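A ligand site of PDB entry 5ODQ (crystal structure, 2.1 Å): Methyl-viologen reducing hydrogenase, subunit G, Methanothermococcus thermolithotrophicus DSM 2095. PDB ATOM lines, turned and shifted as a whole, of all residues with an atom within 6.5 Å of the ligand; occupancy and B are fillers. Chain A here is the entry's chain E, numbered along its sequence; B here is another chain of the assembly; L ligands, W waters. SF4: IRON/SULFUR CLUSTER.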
ATOM      1  N   GLY A  10     -31.707  -7.248 -27.821  1.00  0.00           N
ATOM      2  CA  GLY A  10     -30.881  -6.517 -26.869  1.00  0.00           C
ATOM      3  C   GLY A  10     -30.063  -7.352 -25.896  1.00  0.00           C
ATOM      4  O   GLY A  10     -29.918  -6.952 -24.736  1.00  0.00           O
ATOM      5  N   GLY A  11     -29.528  -8.488 -26.342  1.00  0.00           N
ATOM      6  CA  GLY A  11     -28.713  -9.379 -25.503  1.00  0.00           C
ATOM      7  C   GLY A  11     -27.220  -9.299 -25.807  1.00  0.00           C
ATOM      8  O   GLY A  11     -26.729  -8.253 -26.232  1.00  0.00           O
ATOM      9  N   CYS A  12     -26.484 -10.414 -25.590  1.00  0.00           N
ATOM     10  CA  CYS A  12     -25.031 -10.466 -25.803  1.00  0.00           C
ATOM     11  C   CYS A  12     -24.527 -11.668 -26.649  1.00  0.00           C
ATOM     12  O   CYS A  12     -23.318 -11.766 -26.869  1.00  0.00           O
ATOM     13  CB  CYS A  12     -24.338 -10.442 -24.446  1.00  0.00           C
ATOM     14  SG  CYS A  12     -24.190 -12.069 -23.663  1.00  0.00           S
ATOM     15  N   SER A  13     -25.418 -12.571 -27.106  1.00  0.00           N
ATOM     16  CA  SER A  13     -25.095 -13.783 -27.892  1.00  0.00           C
ATOM     17  C   SER A  13     -24.817 -14.998 -26.984  1.00  0.00           C
ATOM     18  O   SER A  13     -24.686 -16.115 -27.477  1.00  0.00           O
ATOM     19  CB  SER A  13     -23.920 -13.575 -28.851  1.00  0.00           C
ATOM     20  OG  SER A  13     -22.659 -13.898 -28.275  1.00  0.00           O
ATOM     21  N   GLY A  14     -24.734 -14.766 -25.663  1.00  0.00           N
ATOM     22  CA  GLY A  14     -24.466 -15.817 -24.679  1.00  0.00           C
ATOM     23  C   GLY A  14     -25.416 -16.994 -24.736  1.00  0.00           C
ATOM     24  O   GLY A  14     -24.996 -18.132 -24.508  1.00  0.00           O
ATOM     25  N   CYS A  15     -26.702 -16.749 -25.025  1.00  0.00           N
ATOM     26  CA  CYS A  15     -27.677 -17.830 -25.114  1.00  0.00           C
ATOM     27  C   CYS A  15     -27.349 -18.645 -26.365  1.00  0.00           C
ATOM     28  O   CYS A  15     -27.425 -19.873 -26.326  1.00  0.00           O
ATOM     29  CB  CYS A  15     -29.095 -17.289 -25.140  1.00  0.00           C
ATOM     30  SG  CYS A  15     -29.539 -16.314 -23.678  1.00  0.00           S
ATOM     31  N   HIS A  16     -26.979 -17.971 -27.461  1.00  0.00           N
ATOM     32  CA  HIS A  16     -26.616 -18.670 -28.693  1.00  0.00           C
ATOM     33  C   HIS A  16     -25.367 -19.502 -28.437  1.00  0.00           C
ATOM     34  O   HIS A  16     -25.304 -20.642 -28.891  1.00  0.00           O
ATOM     35  CB  HIS A  16     -26.377 -17.696 -29.861  1.00  0.00           C
ATOM     36  CG  HIS A  16     -27.617 -17.307 -30.592  1.00  0.00           C
ATOM     37  ND1 HIS A  16     -28.564 -16.487 -30.025  1.00  0.00           N
ATOM     38  CD2 HIS A  16     -28.030 -17.651 -31.828  1.00  0.00           C
ATOM     39  CE1 HIS A  16     -29.514 -16.339 -30.926  1.00  0.00           C
ATOM     40  NE2 HIS A  16     -29.248 -17.023 -32.029  1.00  0.00           N
ATOM     41  N   GLU A  57     -33.526 -14.436 -28.593  1.00  0.00           N
ATOM     42  CA  GLU A  57     -32.617 -14.036 -27.544  1.00  0.00           C
ATOM     43  C   GLU A  57     -32.695 -12.525 -27.351  1.00  0.00           C
ATOM     44  O   GLU A  57     -32.976 -11.802 -28.299  1.00  0.00           O
ATOM     45  CB  GLU A  57     -31.184 -14.451 -27.923  1.00  0.00           C
ATOM     46  CG  GLU A  57     -30.092 -14.005 -26.975  1.00  0.00           C
ATOM     47  CD  GLU A  57     -28.725 -13.976 -27.621  1.00  0.00           C
ATOM     48  OE1 GLU A  57     -28.342 -12.906 -28.143  1.00  0.00           O
ATOM     49  OE2 GLU A  57     -28.056 -15.036 -27.644  1.00  0.00           O
ATOM     50  N   GLY A  58     -32.465 -12.069 -26.128  1.00  0.00           N
ATOM     51  CA  GLY A  58     -32.478 -10.650 -25.803  1.00  0.00           C
ATOM     52  C   GLY A  58     -33.829 -10.002 -25.612  1.00  0.00           C
ATOM     53  O   GLY A  58     -34.864 -10.516 -26.073  1.00  0.00           O
ATOM     54  N   PHE A  82     -35.800 -16.759 -25.295  1.00  0.00           N
ATOM     55  CA  PHE A  82     -34.558 -17.474 -25.090  1.00  0.00           C
ATOM     56  C   PHE A  82     -33.594 -16.742 -24.194  1.00  0.00           C
ATOM     57  O   PHE A  82     -32.842 -15.890 -24.647  1.00  0.00           O
ATOM     58  CB  PHE A  82     -33.923 -17.760 -26.448  1.00  0.00           C
ATOM     59  CG  PHE A  82     -32.759 -18.726 -26.481  1.00  0.00           C
ATOM     60  CD1 PHE A  82     -32.604 -19.679 -25.496  1.00  0.00           C
ATOM     61  CD2 PHE A  82     -31.851 -18.689 -27.516  1.00  0.00           C
ATOM     62  CE1 PHE A  82     -31.543 -20.563 -25.540  1.00  0.00           C
ATOM     63  CE2 PHE A  82     -30.790 -19.585 -27.554  1.00  0.00           C
ATOM     64  CZ  PHE A  82     -30.643 -20.516 -26.571  1.00  0.00           C
ATOM     65  N   GLY A  83     -33.613 -17.103 -22.910  1.00  0.00           N
ATOM     66  CA  GLY A  83     -32.729 -16.494 -21.938  1.00  0.00           C
ATOM     67  C   GLY A  83     -33.330 -15.374 -21.132  1.00  0.00           C
ATOM     68  O   GLY A  83     -34.363 -14.794 -21.514  1.00  0.00           O
ATOM     69  N   THR A  84     -32.674 -15.071 -20.019  1.00  0.00           N
ATOM     70  CA  THR A  84     -33.056 -14.042 -19.052  1.00  0.00           C
ATOM     71  C   THR A  84     -33.292 -12.679 -19.679  1.00  0.00           C
ATOM     72  O   THR A  84     -34.208 -11.970 -19.255  1.00  0.00           O
ATOM     73  CB  THR A  84     -31.975 -13.996 -17.973  1.00  0.00           C
ATOM     74  OG1 THR A  84     -32.130 -15.153 -17.151  1.00  0.00           O
ATOM     75  CG2 THR A  84     -32.006 -12.736 -17.135  1.00  0.00           C
ATOM     76  N   CYS A  85     -32.496 -12.278 -20.664  1.00  0.00           N
ATOM     77  CA  CYS A  85     -32.720 -10.969 -21.271  1.00  0.00           C
ATOM     78  C   CYS A  85     -34.126 -10.935 -21.900  1.00  0.00           C
ATOM     79  O   CYS A  85     -34.903 -10.041 -21.591  1.00  0.00           O
ATOM     80  CB  CYS A  85     -31.640 -10.640 -22.305  1.00  0.00           C
ATOM     81  SG  CYS A  85     -30.034 -10.194 -21.579  1.00  0.00           S
ATOM     82  N   ALA A  86     -34.445 -11.909 -22.746  1.00  0.00           N
ATOM     83  CA  ALA A  86     -35.754 -11.988 -23.396  1.00  0.00           C
ATOM     84  C   ALA A  86     -36.884 -12.176 -22.388  1.00  0.00           C
ATOM     85  O   ALA A  86     -37.937 -11.553 -22.521  1.00  0.00           O
ATOM     86  CB  ALA A  86     -35.785 -13.149 -24.382  1.00  0.00           C
ATOM     87  N   GLY A  89     -35.634  -9.239 -19.023  1.00  0.00           N
ATOM     88  CA  GLY A  89     -35.000  -7.977 -19.381  1.00  0.00           C
ATOM     89  C   GLY A  89     -33.486  -8.015 -19.343  1.00  0.00           C
ATOM     90  O   GLY A  89     -32.820  -7.405 -20.180  1.00  0.00           O
ATOM     91  N   GLY A  90     -32.930  -8.735 -18.359  1.00  0.00           N
ATOM     92  CA  GLY A  90     -31.489  -8.895 -18.210  1.00  0.00           C
ATOM     93  C   GLY A  90     -30.681  -7.688 -17.757  1.00  0.00           C
ATOM     94  O   GLY A  90     -31.242  -6.630 -17.462  1.00  0.00           O
ATOM     95  N   VAL A  91     -29.346  -7.857 -17.711  1.00  0.00           N
ATOM     96  CA  VAL A  91     -28.375  -6.825 -17.300  1.00  0.00           C
ATOM     97  C   VAL A  91     -28.555  -5.508 -18.061  1.00  0.00           C
ATOM     98  O   VAL A  91     -28.518  -4.445 -17.439  1.00  0.00           O
ATOM     99  CB  VAL A  91     -26.920  -7.350 -17.365  1.00  0.00           C
ATOM    100  CG1 VAL A  91     -25.912  -6.205 -17.300  1.00  0.00           C
ATOM    101  CG2 VAL A  91     -26.667  -8.353 -16.237  1.00  0.00           C
ATOM    102  N   PRO A  92     -28.773  -5.514 -19.394  1.00  0.00           N
ATOM    103  CA  PRO A  92     -28.957  -4.240 -20.100  1.00  0.00           C
ATOM    104  C   PRO A  92     -30.101  -3.421 -19.504  1.00  0.00           C
ATOM    105  O   PRO A  92     -30.129  -2.200 -19.623  1.00  0.00           O
ATOM    106  CB  PRO A  92     -29.244  -4.679 -21.542  1.00  0.00           C
ATOM    107  CG  PRO A  92     -28.582  -6.021 -21.643  1.00  0.00           C
ATOM    108  CD  PRO A  92     -28.869  -6.652 -20.328  1.00  0.00           C
ATOM    109  N   GLY A 148     -32.304 -18.168 -17.614  1.00  0.00           N
ATOM    110  CA  GLY A 148     -30.875 -18.372 -17.445  1.00  0.00           C
ATOM    111  C   GLY A 148     -30.056 -17.355 -18.195  1.00  0.00           C
ATOM    112  O   GLY A 148     -30.451 -16.929 -19.287  1.00  0.00           O
ATOM    113  N   CYS A 149     -28.920 -16.961 -17.624  1.00  0.00           N
ATOM    114  CA  CYS A 149     -28.030 -15.981 -18.243  1.00  0.00           C
ATOM    115  C   CYS A 149     -26.623 -16.570 -18.369  1.00  0.00           C
ATOM    116  O   CYS A 149     -25.712 -16.207 -17.623  1.00  0.00           O
ATOM    117  CB  CYS A 149     -28.008 -14.682 -17.446  1.00  0.00           C
ATOM    118  SG  CYS A 149     -27.000 -13.372 -18.178  1.00  0.00           S
ATOM    119  N   PRO A 150     -26.409 -17.497 -19.317  1.00  0.00           N
ATOM    120  CA  PRO A 150     -27.391 -18.036 -20.258  1.00  0.00           C
ATOM    121  C   PRO A 150     -27.964 -19.331 -19.729  1.00  0.00           C
ATOM    122  O   PRO A 150     -27.443 -19.898 -18.774  1.00  0.00           O
ATOM    123  CB  PRO A 150     -26.538 -18.314 -21.494  1.00  0.00           C
ATOM    124  CG  PRO A 150     -25.163 -18.662 -20.932  1.00  0.00           C
ATOM    125  CD  PRO A 150     -25.092 -18.110 -19.523  1.00  0.00           C
ATOM    126  N   PRO A 151     -29.011 -19.865 -20.344  1.00  0.00           N
ATOM    127  CA  PRO A 151     -29.544 -21.138 -19.862  1.00  0.00           C
ATOM    128  C   PRO A 151     -28.569 -22.272 -20.112  1.00  0.00           C
ATOM    129  O   PRO A 151     -27.866 -22.269 -21.104  1.00  0.00           O
ATOM    130  CB  PRO A 151     -30.829 -21.312 -20.687  1.00  0.00           C
ATOM    131  CG  PRO A 151     -31.101 -19.982 -21.307  1.00  0.00           C
ATOM    132  CD  PRO A 151     -29.762 -19.372 -21.506  1.00  0.00           C
ATOM    133  N   CYS A 238     -29.220 -14.737 -11.644  1.00  0.00           N
ATOM    134  CA  CYS A 238     -29.285 -14.713 -13.101  1.00  0.00           C
ATOM    135  C   CYS A 238     -30.393 -15.580 -13.748  1.00  0.00           C
ATOM    136  O   CYS A 238     -30.782 -15.276 -14.880  1.00  0.00           O
ATOM    137  CB  CYS A 238     -27.918 -15.025 -13.700  1.00  0.00           C
ATOM    138  SG  CYS A 238     -27.699 -16.750 -14.230  1.00  0.00           S
ATOM    139  N   PHE A 287     -30.407  -8.723 -13.002  1.00  0.00           N
ATOM    140  CA  PHE A 287     -30.945  -9.317 -14.225  1.00  0.00           C
ATOM    141  C   PHE A 287     -32.439  -9.191 -14.451  1.00  0.00           C
ATOM    142  O   PHE A 287     -32.926  -9.704 -15.448  1.00  0.00           O
ATOM    143  CB  PHE A 287     -30.657 -10.811 -14.151  1.00  0.00           C
ATOM    144  CG  PHE A 287     -29.209 -11.159 -13.916  1.00  0.00           C
ATOM    145  CD1 PHE A 287     -28.346 -11.333 -14.971  1.00  0.00           C
ATOM    146  CD2 PHE A 287     -28.725 -11.309 -12.630  1.00  0.00           C
ATOM    147  CE1 PHE A 287     -27.013 -11.646 -14.750  1.00  0.00           C
ATOM    148  CE2 PHE A 287     -27.390 -11.626 -12.417  1.00  0.00           C
ATOM    149  CZ  PHE A 287     -26.547 -11.795 -13.481  1.00  0.00           C
ATOM    150  N   ARG B  39     -26.145  -0.620 -25.895  1.00  0.00           N
ATOM    151  CA  ARG B  39     -26.813  -0.891 -24.620  1.00  0.00           C
ATOM    152  C   ARG B  39     -26.482   0.153 -23.531  1.00  0.00           C
ATOM    153  O   ARG B  39     -27.265   0.333 -22.596  1.00  0.00           O
ATOM    154  CB  ARG B  39     -26.509  -2.323 -24.171  1.00  0.00           C
ATOM    155  CG  ARG B  39     -27.278  -3.340 -25.021  1.00  0.00           C
ATOM    156  CD  ARG B  39     -26.756  -4.740 -24.842  1.00  0.00           C
ATOM    157  NE  ARG B  39     -25.371  -4.830 -25.307  1.00  0.00           N
ATOM    158  CZ  ARG B  39     -24.525  -5.785 -24.968  1.00  0.00           C
ATOM    159  NH1 ARG B  39     -24.897  -6.758 -24.146  1.00  0.00           N
ATOM    160  NH2 ARG B  39     -23.287  -5.786 -25.437  1.00  0.00           N
ATOM    161  N   ARG B  59     -21.455  -9.793 -19.340  1.00  0.00           N
ATOM    162  CA  ARG B  59     -22.699  -9.711 -20.101  1.00  0.00           C
ATOM    163  C   ARG B  59     -22.602  -8.752 -21.310  1.00  0.00           C
ATOM    164  O   ARG B  59     -23.616  -8.531 -21.989  1.00  0.00           O
ATOM    165  CB  ARG B  59     -23.894  -9.361 -19.199  1.00  0.00           C
ATOM    166  CG  ARG B  59     -24.498 -10.575 -18.524  1.00  0.00           C
ATOM    167  CD  ARG B  59     -23.720 -11.060 -17.324  1.00  0.00           C
ATOM    168  NE  ARG B  59     -24.202 -12.367 -16.869  1.00  0.00           N
ATOM    169  CZ  ARG B  59     -23.722 -13.020 -15.824  1.00  0.00           C
ATOM    170  NH1 ARG B  59     -22.735 -12.518 -15.105  1.00  0.00           N
ATOM    171  NH2 ARG B  59     -24.228 -14.204 -15.495  1.00  0.00           N
ATOM    172  N   ILE B  60     -21.407  -8.198 -21.599  1.00  0.00           N
ATOM    173  CA  ILE B  60     -21.228  -7.319 -22.747  1.00  0.00           C
ATOM    174  C   ILE B  60     -21.187  -8.257 -23.942  1.00  0.00           C
ATOM    175  O   ILE B  60     -21.640  -7.900 -25.025  1.00  0.00           O
ATOM    176  CB  ILE B  60     -19.936  -6.470 -22.641  1.00  0.00           C
ATOM    177  CG1 ILE B  60     -20.100  -5.390 -21.562  1.00  0.00           C
ATOM    178  CG2 ILE B  60     -19.592  -5.820 -23.986  1.00  0.00           C
ATOM    179  CD1 ILE B  60     -18.813  -4.688 -21.176  1.00  0.00           C
ATOM    180  N   CYS B  61     -20.660  -9.476 -23.749  1.00  0.00           N
ATOM    181  CA  CYS B  61     -20.585 -10.457 -24.833  1.00  0.00           C
ATOM    182  C   CYS B  61     -20.463 -11.879 -24.298  1.00  0.00           C
ATOM    183  O   CYS B  61     -19.704 -12.143 -23.377  1.00  0.00           O
ATOM    184  CB  CYS B  61     -19.434 -10.126 -25.769  1.00  0.00           C
ATOM    185  SG  CYS B  61     -19.069 -11.440 -26.953  1.00  0.00           S
ATOM    186  N   GLY B  62     -21.218 -12.788 -24.923  1.00  0.00           N
ATOM    187  CA  GLY B  62     -21.258 -14.202 -24.562  1.00  0.00           C
ATOM    188  C   GLY B  62     -20.115 -15.027 -25.121  1.00  0.00           C
ATOM    189  O   GLY B  62     -19.989 -16.201 -24.757  1.00  0.00           O
ATOM    190  N   ILE B 162     -19.523 -19.923 -19.545  1.00  0.00           N
ATOM    191  CA  ILE B 162     -19.953 -18.647 -20.109  1.00  0.00           C
ATOM    192  C   ILE B 162     -20.281 -17.779 -18.897  1.00  0.00           C
ATOM    193  O   ILE B 162     -21.116 -18.158 -18.084  1.00  0.00           O
ATOM    194  CB  ILE B 162     -21.165 -18.812 -21.082  1.00  0.00           C
ATOM    195  CG1 ILE B 162     -20.817 -19.807 -22.213  1.00  0.00           C
ATOM    196  CG2 ILE B 162     -21.563 -17.442 -21.674  1.00  0.00           C
ATOM    197  CD1 ILE B 162     -22.000 -20.222 -23.063  1.00  0.00           C
ATOM    198  N   HIS B 163     -19.595 -16.638 -18.765  1.00  0.00           N
ATOM    199  CA  HIS B 163     -19.733 -15.701 -17.653  1.00  0.00           C
ATOM    200  C   HIS B 163     -19.090 -16.280 -16.395  1.00  0.00           C
ATOM    201  O   HIS B 163     -19.762 -16.645 -15.443  1.00  0.00           O
ATOM    202  CB  HIS B 163     -21.202 -15.288 -17.397  1.00  0.00           C
ATOM    203  CG  HIS B 163     -21.862 -14.678 -18.594  1.00  0.00           C
ATOM    204  ND1 HIS B 163     -21.211 -13.753 -19.387  1.00  0.00           N
ATOM    205  CD2 HIS B 163     -23.099 -14.883 -19.103  1.00  0.00           C
ATOM    206  CE1 HIS B 163     -22.057 -13.431 -20.349  1.00  0.00           C
ATOM    207  NE2 HIS B 163     -23.210 -14.083 -20.218  1.00  0.00           N
HETATM  208 FE1  SF4 L   1     -28.301 -14.627 -22.698  1.00  0.00          FE
HETATM  209 FE2  SF4 L   1     -26.296 -12.771 -22.732  1.00  0.00          FE
HETATM  210 FE3  SF4 L   1     -27.355 -13.542 -20.443  1.00  0.00          FE
HETATM  211 FE4  SF4 L   1     -28.807 -11.989 -22.108  1.00  0.00          FE
HETATM  212  S1  SF4 L   1     -26.864 -11.378 -21.031  1.00  0.00           S
HETATM  213  S2  SF4 L   1     -29.605 -13.836 -21.001  1.00  0.00           S
HETATM  214  S3  SF4 L   1     -28.136 -12.836 -24.128  1.00  0.00           S
HETATM  215  S4  SF4 L   1     -26.193 -14.888 -21.781  1.00  0.00           S
HETATM  216  O   HOH W   1     -28.913 -10.598 -18.672  1.00  0.00           O
HETATM  217  O   HOH W   2     -31.757 -13.676 -23.711  1.00  0.00           O
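The backbone NH (N) of Cys 15 lies close to a sulfur (S4) of the ligand, at 3.8 Å. An iron atom (FE1) of the ligand is bound by the side-chain sulfur (SG) of Cys 15, at 2.3 Å. FE3 of the ligand is bound by SG of Cys 149 (2.3 Å). S3 of the ligand sits close to N of Cys 12. A sulfur (S4) of the ligand sits close to a ring nitrogen (NE2) of His 163 of chain B (3.5 Å). SG of Cys 12 is bound to FE2 of the ligand (2.4 Å). A sulfur (S2) of the ligand lies close to the backbone NH (N) of Thr 84 (3.5 Å). The backbone NH of Cys 85 sits close to a sulfur (S2) of the ligand. FE4 of the ligand is bound by SG of Cys 85 (2.2 Å).
Water W1 bridges N of Val 91 and S1 of the ligand.
N of Cys 149 lies close to SG of Cys 238. O of Arg 59 of chain B lies within hydrogen-bond range of NH1 of Arg 39 of chain B (3.1 Å). N of Gly 89 lies within hydrogen-bond range of O of Thr 84, at 3.1 Å. The backbone carbonyl oxygen of Gly 11 is in hydrogen-bond range of the guanidinium group of Arg 39 of chain B. N of Cys 15 sits at hydrogen-bond distance from OE2 of Glu 57 (3.4 Å). The side-chain carboxylate (OE2) of Glu 57 lies within hydrogen-bond range of a ring nitrogen (ND1) of His 16. O of Cys 149 is in hydrogen-bond range of NH2 of Arg 59 of chain B (3.3 Å). The backbone carbonyl oxygen (O) of Cys 12 sits at hydrogen-bond distance from the backbone NH (N) of Gly 62 of chain B, at 3.0 Å.
A sulfur (S2) of the ligand lies close to the backbone carbonyl oxygen (O) of Gly 148 (3.6 Å). The backbone nitrogen (N) of Pro 150 lies close to a sulfur (S4) of the ligand (3.6 Å). Merely in contact with the ligand: Gly 11 (3.8 Å), Gly 14 (3.5 Å), Glu 57 (3.6 Å) and Arg 59 of chain B (3.5 Å). Hydrophobic or aromatic side chains within 4 Å of the ligand: Pro 150. The nearest printed residue that does not touch the ligand is Gly 83 (4.03 Å).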
